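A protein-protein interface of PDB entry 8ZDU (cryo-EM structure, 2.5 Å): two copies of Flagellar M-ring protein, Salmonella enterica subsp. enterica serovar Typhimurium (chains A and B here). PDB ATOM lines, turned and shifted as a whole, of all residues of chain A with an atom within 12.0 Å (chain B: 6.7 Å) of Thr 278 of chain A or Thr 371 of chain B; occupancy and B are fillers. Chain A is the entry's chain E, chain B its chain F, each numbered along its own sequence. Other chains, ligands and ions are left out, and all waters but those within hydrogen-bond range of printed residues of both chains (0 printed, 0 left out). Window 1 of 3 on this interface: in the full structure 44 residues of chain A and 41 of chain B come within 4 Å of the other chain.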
ATOM      1  N   ASN A 274      35.725  31.284 -11.448  1.00  0.00           N
ATOM      2  CA  ASN A 274      34.302  31.203 -11.139  1.00  0.00           C
ATOM      3  C   ASN A 274      33.552  30.760 -12.389  1.00  0.00           C
ATOM      4  O   ASN A 274      33.665  31.399 -13.441  1.00  0.00           O
ATOM      5  CB  ASN A 274      33.774  32.549 -10.644  1.00  0.00           C
ATOM      6  CG  ASN A 274      34.417  32.985  -9.343  1.00  0.00           C
ATOM      7  OD1 ASN A 274      35.618  32.810  -9.142  1.00  0.00           O
ATOM      8  ND2 ASN A 274      33.618  33.558  -8.451  1.00  0.00           N
ATOM      9  N   LYS A 275      32.790  29.674 -12.273  1.00  0.00           N
ATOM     10  CA  LYS A 275      32.074  29.104 -13.404  1.00  0.00           C
ATOM     11  C   LYS A 275      30.622  28.841 -13.031  1.00  0.00           C
ATOM     12  O   LYS A 275      30.303  28.517 -11.884  1.00  0.00           O
ATOM     13  CB  LYS A 275      32.721  27.796 -13.885  1.00  0.00           C
ATOM     14  CG  LYS A 275      34.221  27.708 -13.663  1.00  0.00           C
ATOM     15  CD  LYS A 275      34.841  26.635 -14.540  1.00  0.00           C
ATOM     16  CE  LYS A 275      36.232  27.034 -15.005  1.00  0.00           C
ATOM     17  NZ  LYS A 275      37.156  25.867 -15.049  1.00  0.00           N
ATOM     18  N   GLU A 276      29.745  28.986 -14.023  1.00  0.00           N
ATOM     19  CA  GLU A 276      28.335  28.653 -13.892  1.00  0.00           C
ATOM     20  C   GLU A 276      27.895  27.922 -15.152  1.00  0.00           C
ATOM     21  O   GLU A 276      28.464  28.111 -16.229  1.00  0.00           O
ATOM     22  CB  GLU A 276      27.472  29.903 -13.671  1.00  0.00           C
ATOM     23  CG  GLU A 276      27.383  30.351 -12.223  1.00  0.00           C
ATOM     24  CD  GLU A 276      26.221  31.293 -11.978  1.00  0.00           C
ATOM     25  OE1 GLU A 276      25.341  31.394 -12.857  1.00  0.00           O
ATOM     26  OE2 GLU A 276      26.188  31.933 -10.906  1.00  0.00           O
ATOM     27  N   GLN A 277      26.872  27.081 -15.014  1.00  0.00           N
ATOM     28  CA  GLN A 277      26.410  26.293 -16.148  1.00  0.00           C
ATOM     29  C   GLN A 277      24.910  26.063 -16.049  1.00  0.00           C
ATOM     30  O   GLN A 277      24.377  25.834 -14.959  1.00  0.00           O
ATOM     31  CB  GLN A 277      27.147  24.950 -16.224  1.00  0.00           C
ATOM     32  CG  GLN A 277      26.864  24.156 -17.487  1.00  0.00           C
ATOM     33  CD  GLN A 277      27.792  22.970 -17.649  1.00  0.00           C
ATOM     34  OE1 GLN A 277      28.779  22.837 -16.926  1.00  0.00           O
ATOM     35  NE2 GLN A 277      27.480  22.099 -18.601  1.00  0.00           N
ATOM     36  N   THR A 278      24.239  26.128 -17.198  1.00  0.00           N
ATOM     37  CA  THR A 278      22.818  25.830 -17.311  1.00  0.00           C
ATOM     38  C   THR A 278      22.607  24.935 -18.523  1.00  0.00           C
ATOM     39  O   THR A 278      23.039  25.273 -19.629  1.00  0.00           O
ATOM     40  CB  THR A 278      21.985  27.109 -17.445  1.00  0.00           C
ATOM     41  OG1 THR A 278      22.130  27.903 -16.262  1.00  0.00           O
ATOM     42  CG2 THR A 278      20.515  26.770 -17.643  1.00  0.00           C
ATOM     43  N   GLU A 279      21.946  23.799 -18.314  1.00  0.00           N
ATOM     44  CA  GLU A 279      21.732  22.814 -19.365  1.00  0.00           C
ATOM     45  C   GLU A 279      20.247  22.519 -19.513  1.00  0.00           C
ATOM     46  O   GLU A 279      19.544  22.309 -18.520  1.00  0.00           O
ATOM     47  CB  GLU A 279      22.493  21.514 -19.075  1.00  0.00           C
ATOM     48  CG  GLU A 279      23.958  21.713 -18.717  1.00  0.00           C
ATOM     49  CD  GLU A 279      24.263  21.351 -17.275  1.00  0.00           C
ATOM     50  OE1 GLU A 279      24.683  20.201 -17.027  1.00  0.00           O
ATOM     51  OE2 GLU A 279      24.084  22.215 -16.392  1.00  0.00           O
ATOM     52  N   GLU A 280      19.779  22.507 -20.760  1.00  0.00           N
ATOM     53  CA  GLU A 280      18.405  22.158 -21.099  1.00  0.00           C
ATOM     54  C   GLU A 280      18.428  21.029 -22.117  1.00  0.00           C
ATOM     55  O   GLU A 280      19.175  21.091 -23.098  1.00  0.00           O
ATOM     56  CB  GLU A 280      17.646  23.365 -21.657  1.00  0.00           C
ATOM     57  CG  GLU A 280      16.143  23.303 -21.449  1.00  0.00           C
ATOM     58  CD  GLU A 280      15.455  24.611 -21.782  1.00  0.00           C
ATOM     59  OE1 GLU A 280      16.122  25.512 -22.331  1.00  0.00           O
ATOM     60  OE2 GLU A 280      14.246  24.738 -21.496  1.00  0.00           O
ATOM     61  N   HIS A 281      17.618  20.000 -21.881  1.00  0.00           N
ATOM     62  CA  HIS A 281      17.583  18.834 -22.751  1.00  0.00           C
ATOM     63  C   HIS A 281      16.141  18.425 -23.008  1.00  0.00           C
ATOM     64  O   HIS A 281      15.267  18.600 -22.155  1.00  0.00           O
ATOM     65  CB  HIS A 281      18.361  17.658 -22.147  1.00  0.00           C
ATOM     66  CG  HIS A 281      19.801  17.963 -21.878  1.00  0.00           C
ATOM     67  ND1 HIS A 281      20.725  18.145 -22.885  1.00  0.00           N
ATOM     68  CD2 HIS A 281      20.476  18.123 -20.715  1.00  0.00           C
ATOM     69  CE1 HIS A 281      21.907  18.401 -22.354  1.00  0.00           C
ATOM     70  NE2 HIS A 281      21.783  18.393 -21.039  1.00  0.00           N
ATOM     71  N   TYR A 282      15.906  17.867 -24.194  1.00  0.00           N
ATOM     72  CA  TYR A 282      14.586  17.408 -24.603  1.00  0.00           C
ATOM     73  C   TYR A 282      14.673  15.978 -25.114  1.00  0.00           C
ATOM     74  O   TYR A 282      15.689  15.565 -25.680  1.00  0.00           O
ATOM     75  CB  TYR A 282      13.983  18.302 -25.699  1.00  0.00           C
ATOM     76  CG  TYR A 282      13.540  19.668 -25.227  1.00  0.00           C
ATOM     77  CD1 TYR A 282      14.433  20.729 -25.173  1.00  0.00           C
ATOM     78  CD2 TYR A 282      12.225  19.898 -24.848  1.00  0.00           C
ATOM     79  CE1 TYR A 282      14.030  21.981 -24.747  1.00  0.00           C
ATOM     80  CE2 TYR A 282      11.812  21.145 -24.422  1.00  0.00           C
ATOM     81  CZ  TYR A 282      12.718  22.183 -24.373  1.00  0.00           C
ATOM     82  OH  TYR A 282      12.312  23.426 -23.948  1.00  0.00           O
ATOM     83  N   ARG A 370      11.142  17.566 -20.831  1.00  0.00           N
ATOM     84  CA  ARG A 370      12.303  18.441 -20.783  1.00  0.00           C
ATOM     85  C   ARG A 370      12.982  18.333 -19.425  1.00  0.00           C
ATOM     86  O   ARG A 370      12.348  18.016 -18.415  1.00  0.00           O
ATOM     87  CB  ARG A 370      11.918  19.899 -21.070  1.00  0.00           C
ATOM     88  CG  ARG A 370      11.277  20.627 -19.904  1.00  0.00           C
ATOM     89  CD  ARG A 370      10.601  21.906 -20.366  1.00  0.00           C
ATOM     90  NE  ARG A 370      11.519  23.038 -20.388  1.00  0.00           N
ATOM     91  CZ  ARG A 370      11.164  24.291 -20.140  1.00  0.00           C
ATOM     92  NH1 ARG A 370       9.916  24.610 -19.836  1.00  0.00           N
ATOM     93  NH2 ARG A 370      12.084  25.250 -20.199  1.00  0.00           N
ATOM     94  N   THR A 371      14.287  18.590 -19.421  1.00  0.00           N
ATOM     95  CA  THR A 371      15.103  18.544 -18.214  1.00  0.00           C
ATOM     96  C   THR A 371      15.982  19.784 -18.157  1.00  0.00           C
ATOM     97  O   THR A 371      16.616  20.145 -19.155  1.00  0.00           O
ATOM     98  CB  THR A 371      15.971  17.282 -18.176  1.00  0.00           C
ATOM     99  OG1 THR A 371      15.155  16.130 -18.426  1.00  0.00           O
ATOM    100  CG2 THR A 371      16.640  17.135 -16.819  1.00  0.00           C
ATOM    101  N   ILE A 372      16.020  20.430 -16.990  1.00  0.00           N
ATOM    102  CA  ILE A 372      16.792  21.649 -16.773  1.00  0.00           C
ATOM    103  C   ILE A 372      17.697  21.441 -15.567  1.00  0.00           C
ATOM    104  O   ILE A 372      17.238  20.993 -14.510  1.00  0.00           O
ATOM    105  CB  ILE A 372      15.881  22.873 -16.556  1.00  0.00           C
ATOM    106  CG1 ILE A 372      14.829  22.964 -17.663  1.00  0.00           C
ATOM    107  CG2 ILE A 372      16.710  24.148 -16.487  1.00  0.00           C
ATOM    108  CD1 ILE A 372      14.151  24.312 -17.755  1.00  0.00           C
ATOM    109  N   ARG A 373      18.979  21.769 -15.722  1.00  0.00           N
ATOM    110  CA  ARG A 373      19.962  21.625 -14.658  1.00  0.00           C
ATOM    111  C   ARG A 373      20.778  22.901 -14.531  1.00  0.00           C
ATOM    112  O   ARG A 373      21.194  23.488 -15.535  1.00  0.00           O
ATOM    113  CB  ARG A 373      20.895  20.435 -14.917  1.00  0.00           C
ATOM    114  CG  ARG A 373      21.468  19.813 -13.655  1.00  0.00           C
ATOM    115  CD  ARG A 373      22.707  18.987 -13.959  1.00  0.00           C
ATOM    116  NE  ARG A 373      23.244  18.351 -12.761  1.00  0.00           N
ATOM    117  CZ  ARG A 373      22.918  17.133 -12.351  1.00  0.00           C
ATOM    118  NH1 ARG A 373      22.055  16.385 -13.020  1.00  0.00           N
ATOM    119  NH2 ARG A 373      23.470  16.652 -11.241  1.00  0.00           N
ATOM    120  N   HIS A 374      21.008  23.327 -13.290  1.00  0.00           N
ATOM    121  CA  HIS A 374      21.809  24.506 -12.989  1.00  0.00           C
ATOM    122  C   HIS A 374      22.939  24.103 -12.055  1.00  0.00           C
ATOM    123  O   HIS A 374      22.706  23.412 -11.058  1.00  0.00           O
ATOM    124  CB  HIS A 374      20.956  25.607 -12.354  1.00  0.00           C
ATOM    125  CG  HIS A 374      21.679  26.907 -12.182  1.00  0.00           C
ATOM    126  ND1 HIS A 374      21.764  27.556 -10.968  1.00  0.00           N
ATOM    127  CD2 HIS A 374      22.351  27.679 -13.068  1.00  0.00           C
ATOM    128  CE1 HIS A 374      22.457  28.670 -11.116  1.00  0.00           C
ATOM    129  NE2 HIS A 374      22.824  28.769 -12.381  1.00  0.00           N
ATOM    130  N   THR A 375      24.159  24.532 -12.374  1.00  0.00           N
ATOM    131  CA  THR A 375      25.333  24.131 -11.610  1.00  0.00           C
ATOM    132  C   THR A 375      26.235  25.331 -11.371  1.00  0.00           C
ATOM    133  O   THR A 375      26.486  26.119 -12.288  1.00  0.00           O
ATOM    134  CB  THR A 375      26.112  23.025 -12.336  1.00  0.00           C
ATOM    135  OG1 THR A 375      25.236  21.928 -12.621  1.00  0.00           O
ATOM    136  CG2 THR A 375      27.265  22.530 -11.476  1.00  0.00           C
ATOM    137  N   LYS A 376      26.715  25.464 -10.137  1.00  0.00           N
ATOM    138  CA  LYS A 376      27.711  26.461  -9.766  1.00  0.00           C
ATOM    139  C   LYS A 376      28.910  25.728  -9.181  1.00  0.00           C
ATOM    140  O   LYS A 376      28.784  25.045  -8.159  1.00  0.00           O
ATOM    141  CB  LYS A 376      27.141  27.466  -8.764  1.00  0.00           C
ATOM    142  CG  LYS A 376      28.192  28.265  -8.012  1.00  0.00           C
ATOM    143  CD  LYS A 376      27.743  29.702  -7.803  1.00  0.00           C
ATOM    144  CE  LYS A 376      28.406  30.316  -6.582  1.00  0.00           C
ATOM    145  NZ  LYS A 376      29.349  31.407  -6.949  1.00  0.00           N
ATOM    146  N   MET A 377      30.064  25.870  -9.825  1.00  0.00           N
ATOM    147  CA  MET A 377      31.240  25.100  -9.457  1.00  0.00           C
ATOM    148  C   MET A 377      31.889  25.659  -8.191  1.00  0.00           C
ATOM    149  O   MET A 377      31.615  26.780  -7.755  1.00  0.00           O
ATOM    150  CB  MET A 377      32.245  25.080 -10.608  1.00  0.00           C
ATOM    151  CG  MET A 377      31.795  24.261 -11.808  1.00  0.00           C
ATOM    152  SD  MET A 377      30.597  25.129 -12.838  1.00  0.00           S
ATOM    153  CE  MET A 377      29.904  23.767 -13.772  1.00  0.00           C
ATOM    154  N   GLU B 279      29.825  31.325 -23.294  1.00  0.00           N
ATOM    155  CA  GLU B 279      29.708  30.361 -24.379  1.00  0.00           C
ATOM    156  C   GLU B 279      28.285  29.826 -24.453  1.00  0.00           C
ATOM    157  O   GLU B 279      27.694  29.462 -23.432  1.00  0.00           O
ATOM    158  CB  GLU B 279      30.690  29.195 -24.200  1.00  0.00           C
ATOM    159  CG  GLU B 279      32.123  29.624 -23.921  1.00  0.00           C
ATOM    160  CD  GLU B 279      32.579  29.262 -22.520  1.00  0.00           C
ATOM    161  OE1 GLU B 279      33.198  28.190 -22.354  1.00  0.00           O
ATOM    162  OE2 GLU B 279      32.319  30.048 -21.585  1.00  0.00           O
ATOM    163  N   GLU B 280      27.743  29.785 -25.669  1.00  0.00           N
ATOM    164  CA  GLU B 280      26.426  29.224 -25.943  1.00  0.00           C
ATOM    165  C   GLU B 280      26.567  28.157 -27.017  1.00  0.00           C
ATOM    166  O   GLU B 280      27.226  28.382 -28.036  1.00  0.00           O
ATOM    167  CB  GLU B 280      25.441  30.307 -26.393  1.00  0.00           C
ATOM    168  CG  GLU B 280      23.987  29.985 -26.099  1.00  0.00           C
ATOM    169  CD  GLU B 280      23.072  31.172 -26.325  1.00  0.00           C
ATOM    170  OE1 GLU B 280      23.543  32.193 -26.867  1.00  0.00           O
ATOM    171  OE2 GLU B 280      21.880  31.083 -25.963  1.00  0.00           O
ATOM    172  N   HIS B 281      25.954  26.998 -26.785  1.00  0.00           N
ATOM    173  CA  HIS B 281      26.056  25.878 -27.709  1.00  0.00           C
ATOM    174  C   HIS B 281      24.687  25.241 -27.899  1.00  0.00           C
ATOM    175  O   HIS B 281      23.856  25.234 -26.988  1.00  0.00           O
ATOM    176  CB  HIS B 281      27.056  24.826 -27.212  1.00  0.00           C
ATOM    177  CG  HIS B 281      28.441  25.358 -27.015  1.00  0.00           C
ATOM    178  ND1 HIS B 281      29.252  25.730 -28.065  1.00  0.00           N
ATOM    179  CD2 HIS B 281      29.157  25.585 -25.888  1.00  0.00           C
ATOM    180  CE1 HIS B 281      30.408  26.161 -27.595  1.00  0.00           C
ATOM    181  NE2 HIS B 281      30.376  26.083 -26.277  1.00  0.00           N
ATOM    182  N   TYR B 282      24.468  24.700 -29.096  1.00  0.00           N
ATOM    183  CA  TYR B 282      23.217  24.043 -29.448  1.00  0.00           C
ATOM    184  C   TYR B 282      23.507  22.668 -30.035  1.00  0.00           C
ATOM    185  O   TYR B 282      24.536  22.455 -30.681  1.00  0.00           O
ATOM    186  CB  TYR B 282      22.404  24.865 -30.460  1.00  0.00           C
ATOM    187  CG  TYR B 282      21.774  26.117 -29.895  1.00  0.00           C
ATOM    188  CD1 TYR B 282      22.481  27.311 -29.841  1.00  0.00           C
ATOM    189  CD2 TYR B 282      20.467  26.108 -29.427  1.00  0.00           C
ATOM    190  CE1 TYR B 282      21.905  28.458 -29.329  1.00  0.00           C
ATOM    191  CE2 TYR B 282      19.883  27.251 -28.915  1.00  0.00           C
ATOM    192  CZ  TYR B 282      20.606  28.422 -28.867  1.00  0.00           C
ATOM    193  OH  TYR B 282      20.029  29.563 -28.358  1.00  0.00           O
ATOM    194  N   SER B 283      22.577  21.735 -29.808  1.00  0.00           N
ATOM    195  CA  SER B 283      22.695  20.379 -30.333  1.00  0.00           C
ATOM    196  C   SER B 283      22.052  20.291 -31.707  1.00  0.00           C
ATOM    197  O   SER B 283      20.891  20.697 -31.866  1.00  0.00           O
ATOM    198  CB  SER B 283      22.034  19.377 -29.389  1.00  0.00           C
ATOM    199  OG  SER B 283      22.755  19.269 -28.175  1.00  0.00           O
ATOM    200  N   ASP B 369      17.997  21.680 -27.698  1.00  0.00           N
ATOM    201  CA  ASP B 369      18.763  21.671 -26.460  1.00  0.00           C
ATOM    202  C   ASP B 369      19.889  22.691 -26.543  1.00  0.00           C
ATOM    203  O   ASP B 369      20.595  22.774 -27.552  1.00  0.00           O
ATOM    204  CB  ASP B 369      19.337  20.278 -26.191  1.00  0.00           C
ATOM    205  CG  ASP B 369      18.423  19.168 -26.666  1.00  0.00           C
ATOM    206  OD1 ASP B 369      18.870  18.337 -27.484  1.00  0.00           O
ATOM    207  OD2 ASP B 369      17.257  19.123 -26.221  1.00  0.00           O
ATOM    208  N   ARG B 370      20.055  23.469 -25.475  1.00  0.00           N
ATOM    209  CA  ARG B 370      21.056  24.525 -25.453  1.00  0.00           C
ATOM    210  C   ARG B 370      21.833  24.478 -24.145  1.00  0.00           C
ATOM    211  O   ARG B 370      21.328  24.020 -23.117  1.00  0.00           O
ATOM    212  CB  ARG B 370      20.418  25.908 -25.643  1.00  0.00           C
ATOM    213  CG  ARG B 370      19.745  26.471 -24.405  1.00  0.00           C
ATOM    214  CD  ARG B 370      18.837  27.635 -24.761  1.00  0.00           C
ATOM    215  NE  ARG B 370      19.552  28.905 -24.781  1.00  0.00           N
ATOM    216  CZ  ARG B 370      19.012  30.071 -24.449  1.00  0.00           C
ATOM    217  NH1 ARG B 370      17.752  30.163 -24.056  1.00  0.00           N
ATOM    218  NH2 ARG B 370      19.756  31.172 -24.515  1.00  0.00           N
ATOM    219  N   THR B 371      23.076  24.951 -24.205  1.00  0.00           N
ATOM    220  CA  THR B 371      23.967  24.996 -23.053  1.00  0.00           C
ATOM    221  C   THR B 371      24.630  26.362 -22.985  1.00  0.00           C
ATOM    222  O   THR B 371      25.128  26.864 -23.999  1.00  0.00           O
ATOM    223  CB  THR B 371      25.032  23.896 -23.129  1.00  0.00           C
ATOM    224  OG1 THR B 371      24.402  22.635 -23.388  1.00  0.00           O
ATOM    225  CG2 THR B 371      25.805  23.810 -21.823  1.00  0.00           C
ATOM    226  N   ILE B 372      24.639  26.959 -21.792  1.00  0.00           N
ATOM    227  CA  ILE B 372      25.212  28.279 -21.560  1.00  0.00           C
ATOM    228  C   ILE B 372      26.219  28.180 -20.421  1.00  0.00           C
ATOM    229  O   ILE B 372      25.911  27.618 -19.363  1.00  0.00           O
ATOM    230  CB  ILE B 372      24.129  29.324 -21.228  1.00  0.00           C
ATOM    231  CG1 ILE B 372      23.004  29.280 -22.264  1.00  0.00           C
ATOM    232  CG2 ILE B 372      24.737  30.716 -21.145  1.00  0.00           C
ATOM    233  CD1 ILE B 372      22.107  30.498 -22.248  1.00  0.00           C
ATOM    234  N   ARG B 373      27.414  28.724 -20.636  1.00  0.00           N
ATOM    235  CA  ARG B 373      28.477  28.705 -19.641  1.00  0.00           C
ATOM    236  C   ARG B 373      29.078  30.095 -19.498  1.00  0.00           C
ATOM    237  O   ARG B 373      29.322  30.781 -20.494  1.00  0.00           O
ATOM    238  CB  ARG B 373      29.573  27.700 -20.015  1.00  0.00           C
ATOM    239  CG  ARG B 373      30.326  27.133 -18.822  1.00  0.00           C
ATOM    240  CD  ARG B 373      31.660  26.540 -19.241  1.00  0.00           C
ATOM    241  NE  ARG B 373      32.374  25.955 -18.111  1.00  0.00           N
ATOM    242  CZ  ARG B 373      32.280  24.685 -17.742  1.00  0.00           C
ATOM    243  NH1 ARG B 373      31.507  23.831 -18.393  1.00  0.00           N
ATOM    244  NH2 ARG B 373      32.978  24.261 -16.693  1.00  0.00           N
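The backbone NH (N) of Glu 280 of chain A is in hydrogen-bond range of the backbone carbonyl oxygen (O) of Arg 370 of chain B, 3.2 Å away.
N of Thr 278 of chain A is in hydrogen-bond range of O of Ile 372 of chain B, at 3.1 Å.
N of Tyr 282 of chain A lies within hydrogen-bond range of OD2 of Asp 369 of chain B.
The guanidinium group (NH1) of Arg 373 of chain B is in hydrogen-bond range of the side-chain amide oxygen (OE1) of Gln 277 of chain A (3.3 Å).
The backbone carbonyl oxygen (O) of His 281 of chain A is in hydrogen-bond range of the backbone NH (N) of Thr 371 of chain A, at 2.9 Å.
O of Arg 373 of chain A sits at hydrogen-bond distance from N of Glu 279 of chain A, 2.9 Å away.
N of Glu 279 of chain B lies within hydrogen-bond range of O of Arg 373 of chain B.
N of Thr 375 of chain A lies within hydrogen-bond range of O of Gln 277 of chain A (2.9 Å).
The backbone carbonyl oxygen (O) of Asp 369 of chain B is in hydrogen-bond range of the backbone NH (N) of Ser 283 of chain B (3.2 Å).
The backbone carbonyl oxygen of Lys 275 of chain A is in hydrogen-bond range of the backbone NH of Met 377 of chain A (3.4 Å).
Lys 275 of chain A touches Arg 373 of chain B.
CG of Arg 373 of chain B touches O of Glu 276 of chain A, 3.3 Å away.
Ile 372 of chain B touches Gln 277 of chain A (O to CA, 3.5 Å).
Thr 278 of chain A touches Thr 371 of chain B.
Glu 279 of chain A touches Arg 370 of chain B.
Asp 369 of chain B touches Glu 280 of chain A (CB to O, 3.2 Å).
OD2 of Asp 369 of chain B touches C of His 281 of chain A, 3.5 Å away.
Asn 274 of chain A touches none of the printed residues of chain B.
Of the printed residues of chain B, Lys 275 of chain A touches Arg 373.
Thr 278 of chain A touches just these residues of chain B: Thr 371 and Ile 372.
Of the printed residues of chain B, Glu 279 of chain A touches Arg 370.
Thr 375 of chain A touches none of the printed residues of chain B.
No residue of chain A comes within 4 Å of Glu 280 of chain B.
No residue of chain A comes within 4 Å of Tyr 282 of chain B.
Of the printed residues of chain A, Thr 371 of chain B touches Thr 278.
The nearest residue of chain B that does not touch Thr 278 of chain A is Arg 370 of chain B (4.1 Å).
The nearest printed residue of chain A that does not touch Thr 371 of chain B is Gln 277 of chain A (4.01 Å).
Of the 10 printed residues of chain B, 5 touch a printed residue of chain A.
Along chain A the printed residues that touch a printed residue of chain B span positions 275 to 282.
Glu 279 of chain A touches Arg 370 of chain B, but with the chains exchanged Arg 370 of chain A does not touch Glu 279 of chain B (16.5 Å).
Glu 280 of chain A touches Arg 370 of chain B, but with the chains exchanged Arg 370 of chain A does not touch Glu 280 of chain B (12.8 Å).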
